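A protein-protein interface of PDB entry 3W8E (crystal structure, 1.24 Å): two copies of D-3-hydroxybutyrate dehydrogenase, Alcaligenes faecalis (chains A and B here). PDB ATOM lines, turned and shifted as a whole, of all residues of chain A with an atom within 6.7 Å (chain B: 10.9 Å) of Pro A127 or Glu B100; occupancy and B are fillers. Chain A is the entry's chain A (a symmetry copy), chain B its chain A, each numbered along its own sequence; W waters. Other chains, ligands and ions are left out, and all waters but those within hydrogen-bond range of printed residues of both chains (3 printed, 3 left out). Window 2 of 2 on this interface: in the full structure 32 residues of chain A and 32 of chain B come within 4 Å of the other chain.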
ATOM      1  N   ARG A  71      35.488  34.384 -23.889  1.00  0.00           N
ATOM      2  CA  ARG A  71      34.110  34.755 -23.650  1.00  0.00           C
ATOM      3  C   ARG A  71      33.740  35.920 -24.643  1.00  0.00           C
ATOM      4  O   ARG A  71      32.630  35.933 -25.203  1.00  0.00           O
ATOM      5  CB  ARG A  71      33.844  35.168 -22.209  1.00  0.00           C
ATOM      6  CG  ARG A  71      33.973  33.889 -21.352  1.00  0.00           C
ATOM      7  CD  ARG A  71      34.116  34.233 -19.885  1.00  0.00           C
ATOM      8  NE  ARG A  71      34.137  32.977 -19.075  1.00  0.00           N
ATOM      9  CZ  ARG A  71      33.079  32.429 -18.469  1.00  0.00           C
ATOM     10  NH1 ARG A  71      31.893  33.007 -18.363  1.00  0.00           N
ATOM     11  NH2 ARG A  71      33.260  31.234 -17.907  1.00  0.00           N
ATOM     12  N   PHE A 119      35.552  25.211 -21.423  1.00  0.00           N
ATOM     13  CA  PHE A 119      34.668  25.702 -20.406  1.00  0.00           C
ATOM     14  C   PHE A 119      34.218  27.140 -20.711  1.00  0.00           C
ATOM     15  O   PHE A 119      33.027  27.431 -20.684  1.00  0.00           O
ATOM     16  CB  PHE A 119      35.373  25.665 -19.015  1.00  0.00           C
ATOM     17  CG  PHE A 119      34.693  26.476 -17.989  1.00  0.00           C
ATOM     18  CD1 PHE A 119      33.458  26.001 -17.407  1.00  0.00           C
ATOM     19  CD2 PHE A 119      35.288  27.619 -17.503  1.00  0.00           C
ATOM     20  CE1 PHE A 119      32.859  26.880 -16.434  1.00  0.00           C
ATOM     21  CE2 PHE A 119      34.601  28.408 -16.492  1.00  0.00           C
ATOM     22  CZ  PHE A 119      33.456  27.974 -16.020  1.00  0.00           C
ATOM     23  N   THR A 122      31.910  27.337 -23.835  1.00  0.00           N
ATOM     24  CA  THR A 122      30.590  26.752 -23.532  1.00  0.00           C
ATOM     25  C   THR A 122      29.774  27.723 -22.675  1.00  0.00           C
ATOM     26  O   THR A 122      28.580  27.873 -22.867  1.00  0.00           O
ATOM     27  CB  THR A 122      30.854  25.410 -22.815  1.00  0.00           C
ATOM     28  OG1 THR A 122      31.461  24.490 -23.746  1.00  0.00           O
ATOM     29  CG2 THR A 122      29.495  24.766 -22.358  1.00  0.00           C
ATOM     30  N   ALA A 123      30.416  28.222 -21.629  1.00  0.00           N
ATOM     31  CA  ALA A 123      29.707  29.130 -20.713  1.00  0.00           C
ATOM     32  C   ALA A 123      29.128  30.312 -21.443  1.00  0.00           C
ATOM     33  O   ALA A 123      27.998  30.746 -21.143  1.00  0.00           O
ATOM     34  CB  ALA A 123      30.606  29.621 -19.667  1.00  0.00           C
ATOM     35  N   ALA A 124      29.873  30.845 -22.390  1.00  0.00           N
ATOM     36  CA  ALA A 124      29.383  32.022 -23.162  1.00  0.00           C
ATOM     37  C   ALA A 124      28.351  31.621 -24.151  1.00  0.00           C
ATOM     38  O   ALA A 124      27.423  32.401 -24.460  1.00  0.00           O
ATOM     39  CB  ALA A 124      30.617  32.693 -23.919  1.00  0.00           C
ATOM     40  N   ALA A 125      28.373  30.441 -24.733  1.00  0.00           N
ATOM     41  CA  ALA A 125      27.470  30.042 -25.796  1.00  0.00           C
ATOM     42  C   ALA A 125      26.117  29.596 -25.239  1.00  0.00           C
ATOM     43  O   ALA A 125      25.086  29.717 -25.867  1.00  0.00           O
ATOM     44  CB  ALA A 125      28.041  28.915 -26.659  1.00  0.00           C
ATOM     45  N   LEU A 126      26.159  28.948 -24.060  1.00  0.00           N
ATOM     46  CA  LEU A 126      24.949  28.295 -23.524  1.00  0.00           C
ATOM     47  C   LEU A 126      23.797  29.216 -23.416  1.00  0.00           C
ATOM     48  O   LEU A 126      22.687  28.781 -23.789  1.00  0.00           O
ATOM     49  CB  LEU A 126      25.168  27.604 -22.182  1.00  0.00           C
ATOM     50  CG  LEU A 126      25.839  26.221 -22.378  1.00  0.00           C
ATOM     51  CD1 LEU A 126      26.268  25.626 -21.034  1.00  0.00           C
ATOM     52  CD2 LEU A 126      24.879  25.224 -23.034  1.00  0.00           C
ATOM     53  N   PRO A 127      23.909  30.470 -22.905  1.00  0.00           N
ATOM     54  CA  PRO A 127      22.656  31.219 -22.694  1.00  0.00           C
ATOM     55  C   PRO A 127      21.933  31.522 -24.034  1.00  0.00           C
ATOM     56  O   PRO A 127      20.712  31.571 -24.104  1.00  0.00           O
ATOM     57  CB  PRO A 127      23.114  32.496 -22.014  1.00  0.00           C
ATOM     58  CG  PRO A 127      24.384  32.044 -21.272  1.00  0.00           C
ATOM     59  CD  PRO A 127      25.053  31.047 -22.182  1.00  0.00           C
ATOM     60  N   ILE A 128      22.755  31.671 -25.083  1.00  0.00           N
ATOM     61  CA  ILE A 128      22.181  31.919 -26.419  1.00  0.00           C
ATOM     62  C   ILE A 128      21.374  30.737 -26.866  1.00  0.00           C
ATOM     63  O   ILE A 128      20.217  30.778 -27.369  1.00  0.00           O
ATOM     64  CB  ILE A 128      23.366  32.229 -27.393  1.00  0.00           C
ATOM     65  CG1 ILE A 128      24.024  33.480 -26.956  1.00  0.00           C
ATOM     66  CG2 ILE A 128      22.804  32.380 -28.842  1.00  0.00           C
ATOM     67  CD1 ILE A 128      25.441  33.720 -27.565  1.00  0.00           C
ATOM     68  N   MET A 129      22.007  29.526 -26.702  1.00  0.00           N
ATOM     69  CA  MET A 129      21.339  28.260 -27.071  1.00  0.00           C
ATOM     70  C   MET A 129      20.117  27.991 -26.202  1.00  0.00           C
ATOM     71  O   MET A 129      19.076  27.501 -26.675  1.00  0.00           O
ATOM     72  CB  MET A 129      22.338  27.113 -27.032  1.00  0.00           C
ATOM     73  CG  MET A 129      23.468  27.282 -28.020  1.00  0.00           C
ATOM     74  SD  MET A 129      24.624  25.915 -27.751  1.00  0.00           S
ATOM     75  CE  MET A 129      25.738  26.310 -29.140  1.00  0.00           C
ATOM     76  N   GLN A 130      20.192  28.320 -24.949  1.00  0.00           N
ATOM     77  CA  GLN A 130      19.065  28.033 -23.971  1.00  0.00           C
ATOM     78  C   GLN A 130      17.883  28.870 -24.356  1.00  0.00           C
ATOM     79  O   GLN A 130      16.750  28.378 -24.342  1.00  0.00           O
ATOM     80  CB  GLN A 130      19.536  28.351 -22.587  1.00  0.00           C
ATOM     81  CG  GLN A 130      20.508  27.211 -22.105  1.00  0.00           C
ATOM     82  CD  GLN A 130      21.224  27.566 -20.826  1.00  0.00           C
ATOM     83  OE1 GLN A 130      21.886  26.740 -20.128  1.00  0.00           O
ATOM     84  NE2 GLN A 130      21.166  28.840 -20.477  1.00  0.00           N
ATOM     85  N   LYS A 131      18.115  30.082 -24.777  1.00  0.00           N
ATOM     86  CA  LYS A 131      17.008  31.034 -25.193  1.00  0.00           C
ATOM     87  C   LYS A 131      16.324  30.577 -26.450  1.00  0.00           C
ATOM     88  O   LYS A 131      15.110  30.730 -26.635  1.00  0.00           O
ATOM     89  CB  LYS A 131      17.556  32.447 -25.400  1.00  0.00           C
ATOM     90  CG  LYS A 131      16.570  33.473 -25.985  1.00  0.00           C
ATOM     91  CD  LYS A 131      17.174  34.859 -25.754  1.00  0.00           C
ATOM     92  CE  LYS A 131      16.323  36.076 -26.231  1.00  0.00           C
ATOM     93  NZ  LYS A 131      16.083  36.197 -27.698  1.00  0.00           N
ATOM     94  N   GLN A 132      17.012  29.892 -27.335  1.00  0.00           N
ATOM     95  CA  GLN A 132      16.305  29.465 -28.533  1.00  0.00           C
ATOM     96  C   GLN A 132      15.874  28.030 -28.502  1.00  0.00           C
ATOM     97  O   GLN A 132      15.122  27.568 -29.391  1.00  0.00           O
ATOM     98  CB  GLN A 132      17.198  29.675 -29.639  1.00  0.00           C
ATOM     99  CG  GLN A 132      18.412  28.772 -29.569  1.00  0.00           C
ATOM    100  CD  GLN A 132      19.587  29.311 -30.402  1.00  0.00           C
ATOM    101  OE1 GLN A 132      20.634  28.622 -30.665  1.00  0.00           O
ATOM    102  NE2 GLN A 132      19.449  30.554 -30.804  1.00  0.00           N
ATOM    103  N   GLU A 172      23.436  19.184 -17.619  1.00  0.00           N
ATOM    104  CA  GLU A 172      22.790  20.488 -17.199  1.00  0.00           C
ATOM    105  C   GLU A 172      21.798  20.936 -18.204  1.00  0.00           C
ATOM    106  O   GLU A 172      20.927  21.743 -17.868  1.00  0.00           O
ATOM    107  CB  GLU A 172      23.881  21.539 -17.061  1.00  0.00           C
ATOM    108  CG  GLU A 172      24.770  21.266 -15.832  1.00  0.00           C
ATOM    109  CD  GLU A 172      25.795  22.386 -15.519  1.00  0.00           C
ATOM    110  OE1 GLU A 172      25.705  23.472 -16.157  1.00  0.00           O
ATOM    111  OE2 GLU A 172      26.604  22.248 -14.617  1.00  0.00           O
ATOM    112  N   ASN A 173      21.943  20.505 -19.421  1.00  0.00           N
ATOM    113  CA  ASN A 173      21.127  20.949 -20.524  1.00  0.00           C
ATOM    114  C   ASN A 173      20.201  19.919 -21.084  1.00  0.00           C
ATOM    115  O   ASN A 173      19.556  20.088 -22.109  1.00  0.00           O
ATOM    116  CB  ASN A 173      21.973  21.613 -21.552  1.00  0.00           C
ATOM    117  CG  ASN A 173      22.550  22.873 -20.998  1.00  0.00           C
ATOM    118  OD1 ASN A 173      23.708  22.890 -20.562  1.00  0.00           O
ATOM    119  ND2 ASN A 173      21.817  23.947 -20.903  1.00  0.00           N
ATOM    120  N   LYS A 176      16.736  20.262 -23.039  1.00  0.00           N
ATOM    121  CA  LYS A 176      16.509  21.682 -23.444  1.00  0.00           C
ATOM    122  C   LYS A 176      16.617  21.794 -24.950  1.00  0.00           C
ATOM    123  O   LYS A 176      16.532  22.972 -25.444  1.00  0.00           O
ATOM    124  CB  LYS A 176      17.448  22.592 -22.705  1.00  0.00           C
ATOM    125  CG  LYS A 176      17.272  22.616 -21.268  1.00  0.00           C
ATOM    126  CD  LYS A 176      18.300  23.606 -20.690  1.00  0.00           C
ATOM    127  CE  LYS A 176      18.333  23.559 -19.145  1.00  0.00           C
ATOM    128  NZ  LYS A 176      19.424  24.527 -18.630  1.00  0.00           N
ATOM    129  N   HIS B  95      32.850  23.550  -5.615  1.00  0.00           N
ATOM    130  CA  HIS B  95      31.962  24.685  -5.749  1.00  0.00           C
ATOM    131  C   HIS B  95      30.888  24.268  -6.685  1.00  0.00           C
ATOM    132  O   HIS B  95      31.213  23.733  -7.749  1.00  0.00           O
ATOM    133  CB  HIS B  95      32.700  25.872  -6.320  1.00  0.00           C
ATOM    134  CG  HIS B  95      31.825  27.061  -6.446  1.00  0.00           C
ATOM    135  ND1 HIS B  95      31.529  27.823  -5.315  1.00  0.00           N
ATOM    136  CD2 HIS B  95      31.062  27.491  -7.456  1.00  0.00           C
ATOM    137  CE1 HIS B  95      30.688  28.794  -5.746  1.00  0.00           C
ATOM    138  NE2 HIS B  95      30.342  28.570  -6.984  1.00  0.00           N
ATOM    139  N   THR B  96      29.658  24.405  -6.320  1.00  0.00           N
ATOM    140  CA  THR B  96      28.552  24.028  -7.244  1.00  0.00           C
ATOM    141  C   THR B  96      27.802  25.189  -7.837  1.00  0.00           C
ATOM    142  O   THR B  96      27.385  26.114  -7.138  1.00  0.00           O
ATOM    143  CB  THR B  96      27.560  23.064  -6.539  1.00  0.00           C
ATOM    144  OG1 THR B  96      26.867  23.796  -5.559  1.00  0.00           O
ATOM    145  CG2 THR B  96      28.229  21.982  -5.790  1.00  0.00           C
ATOM    146  N   ALA B  97      27.611  25.161  -9.125  1.00  0.00           N
ATOM    147  CA  ALA B  97      26.870  26.208  -9.887  1.00  0.00           C
ATOM    148  C   ALA B  97      26.693  25.691 -11.294  1.00  0.00           C
ATOM    149  O   ALA B  97      27.587  24.957 -11.748  1.00  0.00           O
ATOM    150  CB  ALA B  97      27.646  27.481  -9.914  1.00  0.00           C
ATOM    151  N   PRO B  98      25.643  26.128 -12.039  1.00  0.00           N
ATOM    152  CA  PRO B  98      25.638  25.673 -13.459  1.00  0.00           C
ATOM    153  C   PRO B  98      26.722  26.408 -14.259  1.00  0.00           C
ATOM    154  O   PRO B  98      27.258  27.457 -13.843  1.00  0.00           O
ATOM    155  CB  PRO B  98      24.239  26.037 -13.938  1.00  0.00           C
ATOM    156  CG  PRO B  98      24.005  27.308 -13.200  1.00  0.00           C
ATOM    157  CD  PRO B  98      24.578  27.138 -11.821  1.00  0.00           C
ATOM    158  N   ILE B  99      27.101  25.803 -15.356  1.00  0.00           N
ATOM    159  CA  ILE B  99      28.243  26.316 -16.135  1.00  0.00           C
ATOM    160  C   ILE B  99      28.154  27.788 -16.444  1.00  0.00           C
ATOM    161  O   ILE B  99      29.179  28.479 -16.269  1.00  0.00           O
ATOM    162  CB  ILE B  99      28.390  25.493 -17.437  1.00  0.00           C
ATOM    163  CG1 ILE B  99      28.849  24.054 -17.100  1.00  0.00           C
ATOM    164  CG2 ILE B  99      29.381  26.131 -18.376  1.00  0.00           C
ATOM    165  CD1 ILE B  99      28.675  23.050 -18.271  1.00  0.00           C
ATOM    166  N   GLU B 100      27.057  28.226 -16.976  1.00  0.00           N
ATOM    167  CA  GLU B 100      26.933  29.650 -17.392  1.00  0.00           C
ATOM    168  C   GLU B 100      27.035  30.630 -16.252  1.00  0.00           C
ATOM    169  O   GLU B 100      27.252  31.837 -16.525  1.00  0.00           O
ATOM    170  CB  GLU B 100      25.725  29.881 -18.238  1.00  0.00           C
ATOM    171  CG  GLU B 100      24.374  29.655 -17.495  1.00  0.00           C
ATOM    172  CD  GLU B 100      23.895  28.197 -17.443  1.00  0.00           C
ATOM    173  OE1 GLU B 100      24.673  27.278 -17.719  1.00  0.00           O
ATOM    174  OE2 GLU B 100      22.720  27.979 -17.170  1.00  0.00           O
ATOM    175  N   GLU B 101      26.909  30.208 -15.013  1.00  0.00           N
ATOM    176  CA  GLU B 101      26.998  30.994 -13.775  1.00  0.00           C
ATOM    177  C   GLU B 101      28.270  30.646 -12.973  1.00  0.00           C
ATOM    178  O   GLU B 101      28.457  31.139 -11.835  1.00  0.00           O
ATOM    179  CB  GLU B 101      25.792  30.660 -12.776  1.00  0.00           C
ATOM    180  CG  GLU B 101      24.466  31.191 -13.178  1.00  0.00           C
ATOM    181  CD  GLU B 101      23.420  30.584 -12.252  1.00  0.00           C
ATOM    182  OE1 GLU B 101      23.657  30.621 -11.021  1.00  0.00           O
ATOM    183  OE2 GLU B 101      22.403  30.051 -12.741  1.00  0.00           O
ATOM    184  N   PHE B 102      29.119  29.734 -13.440  1.00  0.00           N
ATOM    185  CA  PHE B 102      30.164  29.196 -12.631  1.00  0.00           C
ATOM    186  C   PHE B 102      31.241  30.213 -12.543  1.00  0.00           C
ATOM    187  O   PHE B 102      31.750  30.649 -13.579  1.00  0.00           O
ATOM    188  CB  PHE B 102      30.707  27.910 -13.296  1.00  0.00           C
ATOM    189  CG  PHE B 102      31.415  27.030 -12.314  1.00  0.00           C
ATOM    190  CD1 PHE B 102      30.736  25.964 -11.703  1.00  0.00           C
ATOM    191  CD2 PHE B 102      32.732  27.274 -11.879  1.00  0.00           C
ATOM    192  CE1 PHE B 102      31.355  25.177 -10.779  1.00  0.00           C
ATOM    193  CE2 PHE B 102      33.354  26.462 -10.976  1.00  0.00           C
ATOM    194  CZ  PHE B 102      32.654  25.446 -10.369  1.00  0.00           C
ATOM    195  N   PRO B 103      31.686  30.660 -11.347  1.00  0.00           N
ATOM    196  CA  PRO B 103      32.650  31.766 -11.342  1.00  0.00           C
ATOM    197  C   PRO B 103      33.954  31.370 -11.965  1.00  0.00           C
ATOM    198  O   PRO B 103      34.502  30.315 -11.672  1.00  0.00           O
ATOM    199  CB  PRO B 103      32.822  31.990  -9.807  1.00  0.00           C
ATOM    200  CG  PRO B 103      31.522  31.562  -9.249  1.00  0.00           C
ATOM    201  CD  PRO B 103      31.145  30.334 -10.030  1.00  0.00           C
ATOM    202  N   VAL B 104      34.539  32.245 -12.770  1.00  0.00           N
ATOM    203  CA  VAL B 104      35.785  32.000 -13.398  1.00  0.00           C
ATOM    204  C   VAL B 104      36.878  31.778 -12.406  1.00  0.00           C
ATOM    205  O   VAL B 104      37.745  30.873 -12.543  1.00  0.00           O
ATOM    206  CB  VAL B 104      36.113  33.176 -14.420  1.00  0.00           C
ATOM    207  CG1 VAL B 104      37.551  33.157 -14.820  1.00  0.00           C
ATOM    208  CG2 VAL B 104      35.200  33.131 -15.595  1.00  0.00           C
ATOM    209  N   TRP B 107      36.448  28.221 -11.109  1.00  0.00           N
ATOM    210  CA  TRP B 107      37.056  27.301 -12.135  1.00  0.00           C
ATOM    211  C   TRP B 107      38.535  27.255 -11.961  1.00  0.00           C
ATOM    212  O   TRP B 107      39.179  26.177 -11.805  1.00  0.00           O
ATOM    213  CB  TRP B 107      36.657  27.732 -13.544  1.00  0.00           C
ATOM    214  CG  TRP B 107      37.421  26.995 -14.614  1.00  0.00           C
ATOM    215  CD1 TRP B 107      38.612  27.328 -15.129  1.00  0.00           C
ATOM    216  CD2 TRP B 107      37.056  25.749 -15.225  1.00  0.00           C
ATOM    217  NE1 TRP B 107      39.035  26.379 -16.087  1.00  0.00           N
ATOM    218  CE2 TRP B 107      38.080  25.381 -16.073  1.00  0.00           C
ATOM    219  CE3 TRP B 107      35.922  24.920 -15.115  1.00  0.00           C
ATOM    220  CZ2 TRP B 107      38.071  24.183 -16.830  1.00  0.00           C
ATOM    221  CZ3 TRP B 107      35.971  23.739 -15.960  1.00  0.00           C
ATOM    222  CH2 TRP B 107      37.018  23.410 -16.692  1.00  0.00           C
ATOM    223  N   VAL B 150      25.301  17.246 -12.478  1.00  0.00           N
ATOM    224  CA  VAL B 150      25.070  18.655 -12.823  1.00  0.00           C
ATOM    225  C   VAL B 150      25.776  19.554 -11.815  1.00  0.00           C
ATOM    226  O   VAL B 150      26.001  19.246 -10.683  1.00  0.00           O
ATOM    227  CB  VAL B 150      23.526  18.989 -12.810  1.00  0.00           C
ATOM    228  CG1 VAL B 150      22.794  18.227 -13.907  1.00  0.00           C
ATOM    229  CG2 VAL B 150      22.835  18.700 -11.461  1.00  0.00           C
ATOM    230  N   ASN B 151      26.117  20.762 -12.301  1.00  0.00           N
ATOM    231  CA  ASN B 151      26.572  21.886 -11.484  1.00  0.00           C
ATOM    232  C   ASN B 151      27.952  21.690 -10.905  1.00  0.00           C
ATOM    233  O   ASN B 151      28.375  22.435 -10.020  1.00  0.00           O
ATOM    234  CB  ASN B 151      25.527  22.291 -10.446  1.00  0.00           C
ATOM    235  CG  ASN B 151      24.225  22.687 -11.094  1.00  0.00           C
ATOM    236  OD1 ASN B 151      24.119  23.025 -12.188  1.00  0.00           O
ATOM    237  ND2 ASN B 151      23.166  22.447 -10.309  1.00  0.00           N
ATOM    238  N   LYS B 152      28.701  20.751 -11.484  1.00  0.00           N
ATOM    239  CA  LYS B 152      30.033  20.457 -10.958  1.00  0.00           C
ATOM    240  C   LYS B 152      31.024  20.443 -12.079  1.00  0.00           C
ATOM    241  O   LYS B 152      31.966  19.660 -12.134  1.00  0.00           O
ATOM    242  CB  LYS B 152      30.054  19.134 -10.200  1.00  0.00           C
ATOM    243  CG  LYS B 152      29.280  19.270  -8.875  1.00  0.00           C
ATOM    244  CD  LYS B 152      29.307  17.921  -8.064  1.00  0.00           C
ATOM    245  CE  LYS B 152      28.677  18.221  -6.712  1.00  0.00           C
ATOM    246  NZ  LYS B 152      28.593  16.981  -5.908  1.00  0.00           N
ATOM    247  N   SER B 153      30.860  21.375 -13.055  1.00  0.00           N
ATOM    248  CA  SER B 153      31.762  21.374 -14.236  1.00  0.00           C
ATOM    249  C   SER B 153      33.232  21.374 -13.864  1.00  0.00           C
ATOM    250  O   SER B 153      34.020  20.534 -14.377  1.00  0.00           O
ATOM    251  CB  SER B 153      31.468  22.527 -15.118  1.00  0.00           C
ATOM    252  OG  SER B 153      31.502  23.790 -14.457  1.00  0.00           O
ATOM    253  N   ALA B 154      33.696  22.311 -12.988  1.00  0.00           N
ATOM    254  CA  ALA B 154      35.111  22.388 -12.767  1.00  0.00           C
ATOM    255  C   ALA B 154      35.642  21.113 -12.068  1.00  0.00           C
ATOM    256  O   ALA B 154      36.715  20.639 -12.318  1.00  0.00           O
ATOM    257  CB  ALA B 154      35.455  23.608 -11.850  1.00  0.00           C
HETATM  258  O   HOH W   1      30.990  30.683 -16.216  1.00  0.00           O
HETATM  259  O   HOH W   2      28.851  23.382 -13.601  1.00  0.00           O
HETATM  260  O   HOH W   3      21.789  25.288 -16.917  1.00  0.00           O
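The backbone NH (N) of Ile B99 lies within hydrogen-bond range of the side-chain carboxylate (OE1) of Glu A172 (2.8 Å).
The side-chain carboxylate (OE2) of Glu B100 lies close to the side-chain amide oxygen (OE1) of Gln A130 (3.3 Å).
The backbone NH of Asn B151 sits at hydrogen-bond distance from the side-chain carboxylate of Glu A172, 2.8 Å away.
The backbone NH (N) of Ala B97 is in hydrogen-bond range of the backbone carbonyl oxygen (O) of Asn B151 (3.0 Å).
OE1 of Gln A130 sits at hydrogen-bond distance from ND2 of Asn A173, at 2.9 Å.
The side-chain amino group of Lys A176 sits at hydrogen-bond distance from the backbone carbonyl oxygen of Glu A172 (3.3 Å).
Among the printed residues, pairs that only touch across the chains: Phe A119 with Trp B107, Glu A172 with Pro B98, Arg A71 with Val B104, Ala A123 with Glu B100, Ala A123 with Ile B99, Phe A119 with Phe B102, Glu A172 with Val B150, Phe A119 with Ser B153 and Pro A127 with Glu B100.
Of the printed residues of chain B, Pro A127 touches Glu B100.
Printed residues of chain A within 4 Å of Glu B100: Ala A123, Pro A127 and Gln A130.
Ala A124 touches none of the printed residues of chain B.
No residue of chain B comes within 4 Å of Ala A125.
No residue of chain B comes within 4 Å of Leu A126.
Ile A128 touches none of the printed residues of chain B.
Gln A130 touches one residue of chain B.
Printed residues of chain A within 4 Å of Ser B153: Phe A119.
Printed residues of chain B within 4 Å of Arg A71: Val B104.
Printed residues of chain A within 4 Å of Pro B98: Glu A172.
Of the printed residues of chain A, Phe B102 touches Phe A119 (3.9 Å).
Of the printed residues of chain A, Ile B99 touches Ala A123 and Glu A172.
The nearest residue of chain A that does not touch Glu B100 is Leu A126 (4.03 Å).
The nearest printed residue of chain A that does not touch Val B104 is Phe A119 (4.8 Å).
Of the 16 printed residues of chain B, 9 touch a printed residue of chain A.
Hydrophobic or aromatic side chains of chain B within 4 Å of the printed part of chain A: Pro B98, Ile B99, Phe B102, Val B104, Trp B107 and Val B150.
Among the printed residues, 12 pairs touch across the chains.
Among the printed residues, no Asp or Glu carboxylate lies within 4 Å of a Lys or Arg side-chain nitrogen of the other chain.
No position is printed for both chains.
Water W2 lies within hydrogen-bond range of the side-chain carboxylate (OE2) of Glu A172, the backbone carbonyl oxygen (O) of Ala B97, the side-chain hydroxyl (OG) of Ser B153, the backbone NH (N) of Lys B152 and the backbone NH (N) of Ile B99.
Water W1 lies within hydrogen-bond range of the backbone carbonyl oxygen (O) of Phe B102 (2.7 Å), the backbone carbonyl oxygen (O) of Ile B99 (2.9 Å) and the guanidinium group (NH2) of Arg A71 (2.9 Å).
Water W3 bridges the side-chain carboxylate of Glu B100 (2.9 Å) and the side-chain amino group of Lys A176 (3.0 Å).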
